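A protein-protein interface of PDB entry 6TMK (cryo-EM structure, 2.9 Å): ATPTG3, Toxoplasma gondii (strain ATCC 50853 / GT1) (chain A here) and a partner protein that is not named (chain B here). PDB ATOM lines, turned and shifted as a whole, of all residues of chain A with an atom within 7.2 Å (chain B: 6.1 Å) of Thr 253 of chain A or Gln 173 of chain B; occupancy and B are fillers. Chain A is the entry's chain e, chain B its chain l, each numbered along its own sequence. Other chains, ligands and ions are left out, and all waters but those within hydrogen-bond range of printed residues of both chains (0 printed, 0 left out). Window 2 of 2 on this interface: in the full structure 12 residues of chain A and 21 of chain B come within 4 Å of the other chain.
Printed residues of chain B that touch a printed residue of chain A: Leu 74, Leu 169, Gln 172, Gln 173 and Ala 176. Hydrophobic or aromatic side chains of chain A that line the printed part of chain B: Pro 252. Along chain A the printed residues that touch a printed residue of chain B span positions 251 to 254. Among the printed residues, 8 pairs touch across the chains.
Printed residues of chain A within 4 Å of Gln 173 of chain B: Pro 252 and Thr 253. Printed residues of chain B within 4 Å of Val 251 of chain A: Leu 74. Of the printed residues of chain B, Pro 252 of chain A touches Leu 74, Leu 169, Gln 172 and Gln 173. Of the printed residues of chain A, Leu 74 of chain B touches Val 251 (3.5 Å) and Pro 252 (3.9 Å). Of the printed residues of chain A, Gln 172 of chain B touches Pro 252. Printed residues of chain A within 4 Å of Leu 169 of chain B: Pro 252. The nearest printed residue of chain A that does not touch Gln 173 of chain B is Val 251 of chain A (4.01 Å). The nearest printed residue of chain A that does not touch Gln 172 of chain B is Thr 255 of chain A (4.2 Å).
O of Val 251 of chain A touches CG of Leu 74 of chain B, at 3.5 Å. Pro 252 of chain A touches Leu 74 of chain B. Leu 169 of chain B touches Pro 252 of chain A. Pro 252 of chain A touches Gln 172 of chain B. CA of Pro 252 of chain A touches OE1 of Gln 173 of chain B, at 3.3 Å. Thr 253 of chain A touches Ala 176 of chain B (O to CB, 3.7 Å). Gly 254 of chain A touches Ala 176 of chain B.
O of Pro 252 of chain A is in hydrogen-bond range of OG1 of Thr 255 of chain A.
NE2 of Gln 173 of chain B sits close to OG1 of Thr 253 of chain A, at 3.5 Å.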
ATOM      1  N   VAL A 251     -30.226  26.546  -7.736  1.00  0.00           N
ATOM      2  CA  VAL A 251     -29.321  26.657  -6.597  1.00  0.00           C
ATOM      3  C   VAL A 251     -27.910  26.323  -7.056  1.00  0.00           C
ATOM      4  O   VAL A 251     -27.730  25.406  -7.869  1.00  0.00           O
ATOM      5  CB  VAL A 251     -29.750  25.731  -5.450  1.00  0.00           C
ATOM      6  CG1 VAL A 251     -28.822  25.879  -4.290  1.00  0.00           C
ATOM      7  CG2 VAL A 251     -31.142  26.035  -5.016  1.00  0.00           C
ATOM      8  N   PRO A 252     -26.887  27.020  -6.572  1.00  0.00           N
ATOM      9  CA  PRO A 252     -25.515  26.584  -6.820  1.00  0.00           C
ATOM     10  C   PRO A 252     -24.997  25.623  -5.764  1.00  0.00           C
ATOM     11  O   PRO A 252     -25.345  25.691  -4.585  1.00  0.00           O
ATOM     12  CB  PRO A 252     -24.741  27.907  -6.782  1.00  0.00           C
ATOM     13  CG  PRO A 252     -25.473  28.704  -5.807  1.00  0.00           C
ATOM     14  CD  PRO A 252     -26.919  28.372  -5.996  1.00  0.00           C
ATOM     15  N   THR A 253     -24.140  24.718  -6.215  1.00  0.00           N
ATOM     16  CA  THR A 253     -23.596  23.675  -5.363  1.00  0.00           C
ATOM     17  C   THR A 253     -22.336  24.149  -4.652  1.00  0.00           C
ATOM     18  O   THR A 253     -21.557  24.943  -5.183  1.00  0.00           O
ATOM     19  CB  THR A 253     -23.281  22.425  -6.179  1.00  0.00           C
ATOM     20  OG1 THR A 253     -22.433  22.763  -7.281  1.00  0.00           O
ATOM     21  CG2 THR A 253     -24.540  21.806  -6.696  1.00  0.00           C
ATOM     22  N   GLY A 254     -22.144  23.643  -3.438  1.00  0.00           N
ATOM     23  CA  GLY A 254     -20.923  23.886  -2.705  1.00  0.00           C
ATOM     24  C   GLY A 254     -20.792  25.262  -2.111  1.00  0.00           C
ATOM     25  O   GLY A 254     -19.677  25.679  -1.788  1.00  0.00           O
ATOM     26  N   THR A 255     -21.897  25.979  -1.942  1.00  0.00           N
ATOM     27  CA  THR A 255     -21.876  27.344  -1.450  1.00  0.00           C
ATOM     28  C   THR A 255     -22.239  27.428   0.020  1.00  0.00           C
ATOM     29  O   THR A 255     -22.365  28.532   0.558  1.00  0.00           O
ATOM     30  CB  THR A 255     -22.830  28.209  -2.270  1.00  0.00           C
ATOM     31  OG1 THR A 255     -24.134  27.624  -2.251  1.00  0.00           O
ATOM     32  CG2 THR A 255     -22.349  28.341  -3.687  1.00  0.00           C
ATOM     33  N   VAL A 256     -22.407  26.288   0.679  1.00  0.00           N
ATOM     34  CA  VAL A 256     -22.951  26.251   2.029  1.00  0.00           C
ATOM     35  C   VAL A 256     -22.316  25.085   2.773  1.00  0.00           C
ATOM     36  O   VAL A 256     -22.187  23.982   2.237  1.00  0.00           O
ATOM     37  CB  VAL A 256     -24.487  26.136   1.997  1.00  0.00           C
ATOM     38  CG1 VAL A 256     -25.011  25.661   3.315  1.00  0.00           C
ATOM     39  CG2 VAL A 256     -25.099  27.461   1.643  1.00  0.00           C
ATOM     40  N   LEU B  74     -28.200  23.926 -12.095  1.00  0.00           N
ATOM     41  CA  LEU B  74     -27.663  24.904 -13.030  1.00  0.00           C
ATOM     42  C   LEU B  74     -26.733  24.240 -14.034  1.00  0.00           C
ATOM     43  O   LEU B  74     -26.677  24.640 -15.201  1.00  0.00           O
ATOM     44  CB  LEU B  74     -26.928  25.998 -12.267  1.00  0.00           C
ATOM     45  CG  LEU B  74     -27.689  26.670 -11.130  1.00  0.00           C
ATOM     46  CD1 LEU B  74     -26.801  27.669 -10.445  1.00  0.00           C
ATOM     47  CD2 LEU B  74     -28.945  27.333 -11.616  1.00  0.00           C
ATOM     48  N   SER B  75     -25.989  23.232 -13.594  1.00  0.00           N
ATOM     49  CA  SER B  75     -25.259  22.345 -14.492  1.00  0.00           C
ATOM     50  C   SER B  75     -26.225  21.257 -14.926  1.00  0.00           C
ATOM     51  O   SER B  75     -26.521  20.333 -14.167  1.00  0.00           O
ATOM     52  CB  SER B  75     -24.040  21.757 -13.798  1.00  0.00           C
ATOM     53  OG  SER B  75     -24.442  20.981 -12.689  1.00  0.00           O
ATOM     54  N   GLY B 168     -24.506  35.586 -11.435  1.00  0.00           N
ATOM     55  CA  GLY B 168     -23.913  35.563 -10.111  1.00  0.00           C
ATOM     56  C   GLY B 168     -23.917  34.175  -9.507  1.00  0.00           C
ATOM     57  O   GLY B 168     -22.920  33.726  -8.938  1.00  0.00           O
ATOM     58  N   LEU B 169     -25.046  33.478  -9.620  1.00  0.00           N
ATOM     59  CA  LEU B 169     -25.112  32.108  -9.120  1.00  0.00           C
ATOM     60  C   LEU B 169     -24.111  31.209  -9.836  1.00  0.00           C
ATOM     61  O   LEU B 169     -23.443  30.375  -9.206  1.00  0.00           O
ATOM     62  CB  LEU B 169     -26.523  31.562  -9.280  1.00  0.00           C
ATOM     63  CG  LEU B 169     -27.640  32.276  -8.531  1.00  0.00           C
ATOM     64  CD1 LEU B 169     -28.872  31.425  -8.564  1.00  0.00           C
ATOM     65  CD2 LEU B 169     -27.263  32.588  -7.115  1.00  0.00           C
ATOM     66  N   LEU B 170     -24.001  31.355 -11.155  1.00  0.00           N
ATOM     67  CA  LEU B 170     -23.047  30.541 -11.906  1.00  0.00           C
ATOM     68  C   LEU B 170     -21.617  30.790 -11.438  1.00  0.00           C
ATOM     69  O   LEU B 170     -20.831  29.848 -11.243  1.00  0.00           O
ATOM     70  CB  LEU B 170     -23.179  30.831 -13.397  1.00  0.00           C
ATOM     71  CG  LEU B 170     -24.150  29.953 -14.184  1.00  0.00           C
ATOM     72  CD1 LEU B 170     -25.513  29.987 -13.584  1.00  0.00           C
ATOM     73  CD2 LEU B 170     -24.219  30.407 -15.619  1.00  0.00           C
ATOM     74  N   LYS B 171     -21.260  32.062 -11.258  1.00  0.00           N
ATOM     75  CA  LYS B 171     -19.930  32.398 -10.770  1.00  0.00           C
ATOM     76  C   LYS B 171     -19.694  31.822  -9.382  1.00  0.00           C
ATOM     77  O   LYS B 171     -18.594  31.351  -9.073  1.00  0.00           O
ATOM     78  CB  LYS B 171     -19.754  33.912 -10.758  1.00  0.00           C
ATOM     79  CG  LYS B 171     -19.608  34.534 -12.126  1.00  0.00           C
ATOM     80  CD  LYS B 171     -19.354  36.021 -12.025  1.00  0.00           C
ATOM     81  CE  LYS B 171     -19.053  36.624 -13.383  1.00  0.00           C
ATOM     82  NZ  LYS B 171     -18.459  37.989 -13.280  1.00  0.00           N
ATOM     83  N   GLN B 172     -20.719  31.856  -8.530  1.00  0.00           N
ATOM     84  CA  GLN B 172     -20.601  31.269  -7.201  1.00  0.00           C
ATOM     85  C   GLN B 172     -20.272  29.788  -7.286  1.00  0.00           C
ATOM     86  O   GLN B 172     -19.400  29.289  -6.568  1.00  0.00           O
ATOM     87  CB  GLN B 172     -21.902  31.467  -6.436  1.00  0.00           C
ATOM     88  CG  GLN B 172     -22.088  32.836  -5.871  1.00  0.00           C
ATOM     89  CD  GLN B 172     -23.400  32.984  -5.154  1.00  0.00           C
ATOM     90  OE1 GLN B 172     -24.334  32.221  -5.377  1.00  0.00           O
ATOM     91  NE2 GLN B 172     -23.478  33.965  -4.279  1.00  0.00           N
ATOM     92  N   GLN B 173     -20.973  29.069  -8.158  1.00  0.00           N
ATOM     93  CA  GLN B 173     -20.733  27.638  -8.302  1.00  0.00           C
ATOM     94  C   GLN B 173     -19.305  27.360  -8.762  1.00  0.00           C
ATOM     95  O   GLN B 173     -18.606  26.500  -8.202  1.00  0.00           O
ATOM     96  CB  GLN B 173     -21.747  27.048  -9.275  1.00  0.00           C
ATOM     97  CG  GLN B 173     -21.866  25.551  -9.209  1.00  0.00           C
ATOM     98  CD  GLN B 173     -23.133  25.039  -9.839  1.00  0.00           C
ATOM     99  OE1 GLN B 173     -24.188  25.654  -9.729  1.00  0.00           O
ATOM    100  NE2 GLN B 173     -23.039  23.904 -10.500  1.00  0.00           N
ATOM    101  N   SER B 174     -18.852  28.093  -9.780  1.00  0.00           N
ATOM    102  CA  SER B 174     -17.494  27.907 -10.283  1.00  0.00           C
ATOM    103  C   SER B 174     -16.459  28.165  -9.193  1.00  0.00           C
ATOM    104  O   SER B 174     -15.528  27.369  -8.992  1.00  0.00           O
ATOM    105  CB  SER B 174     -17.261  28.831 -11.472  1.00  0.00           C
ATOM    106  OG  SER B 174     -18.220  28.606 -12.484  1.00  0.00           O
ATOM    107  N   ALA B 175     -16.603  29.286  -8.488  1.00  0.00           N
ATOM    108  CA  ALA B 175     -15.656  29.631  -7.438  1.00  0.00           C
ATOM    109  C   ALA B 175     -15.656  28.588  -6.336  1.00  0.00           C
ATOM    110  O   ALA B 175     -14.601  28.257  -5.784  1.00  0.00           O
ATOM    111  CB  ALA B 175     -15.995  31.002  -6.870  1.00  0.00           C
ATOM    112  N   ALA B 176     -16.830  28.061  -5.997  1.00  0.00           N
ATOM    113  CA  ALA B 176     -16.901  27.054  -4.951  1.00  0.00           C
ATOM    114  C   ALA B 176     -16.135  25.808  -5.353  1.00  0.00           C
ATOM    115  O   ALA B 176     -15.369  25.255  -4.554  1.00  0.00           O
ATOM    116  CB  ALA B 176     -18.357  26.718  -4.656  1.00  0.00           C
ATOM    117  N   VAL B 177     -16.314  25.360  -6.593  1.00  0.00           N
ATOM    118  CA  VAL B 177     -15.587  24.181  -7.055  1.00  0.00           C
ATOM    119  C   VAL B 177     -14.083  24.420  -6.975  1.00  0.00           C
ATOM    120  O   VAL B 177     -13.329  23.590  -6.449  1.00  0.00           O
ATOM    121  CB  VAL B 177     -16.021  23.808  -8.479  1.00  0.00           C
ATOM    122  CG1 VAL B 177     -15.144  22.712  -9.027  1.00  0.00           C
ATOM    123  CG2 VAL B 177     -17.454  23.375  -8.485  1.00  0.00           C
ATOM    124  N   GLU B 178     -13.626  25.563  -7.488  1.00  0.00           N
ATOM    125  CA  GLU B 178     -12.191  25.836  -7.502  1.00  0.00           C
ATOM    126  C   GLU B 178     -11.617  25.870  -6.089  1.00  0.00           C
ATOM    127  O   GLU B 178     -10.587  25.239  -5.801  1.00  0.00           O
ATOM    128  CB  GLU B 178     -11.927  27.156  -8.222  1.00  0.00           C
ATOM    129  CG  GLU B 178     -10.509  27.326  -8.725  1.00  0.00           C
ATOM    130  CD  GLU B 178      -9.609  28.053  -7.741  1.00  0.00           C
ATOM    131  OE1 GLU B 178     -10.052  28.313  -6.604  1.00  0.00           O
ATOM    132  OE2 GLU B 178      -8.456  28.365  -8.104  1.00  0.00           O
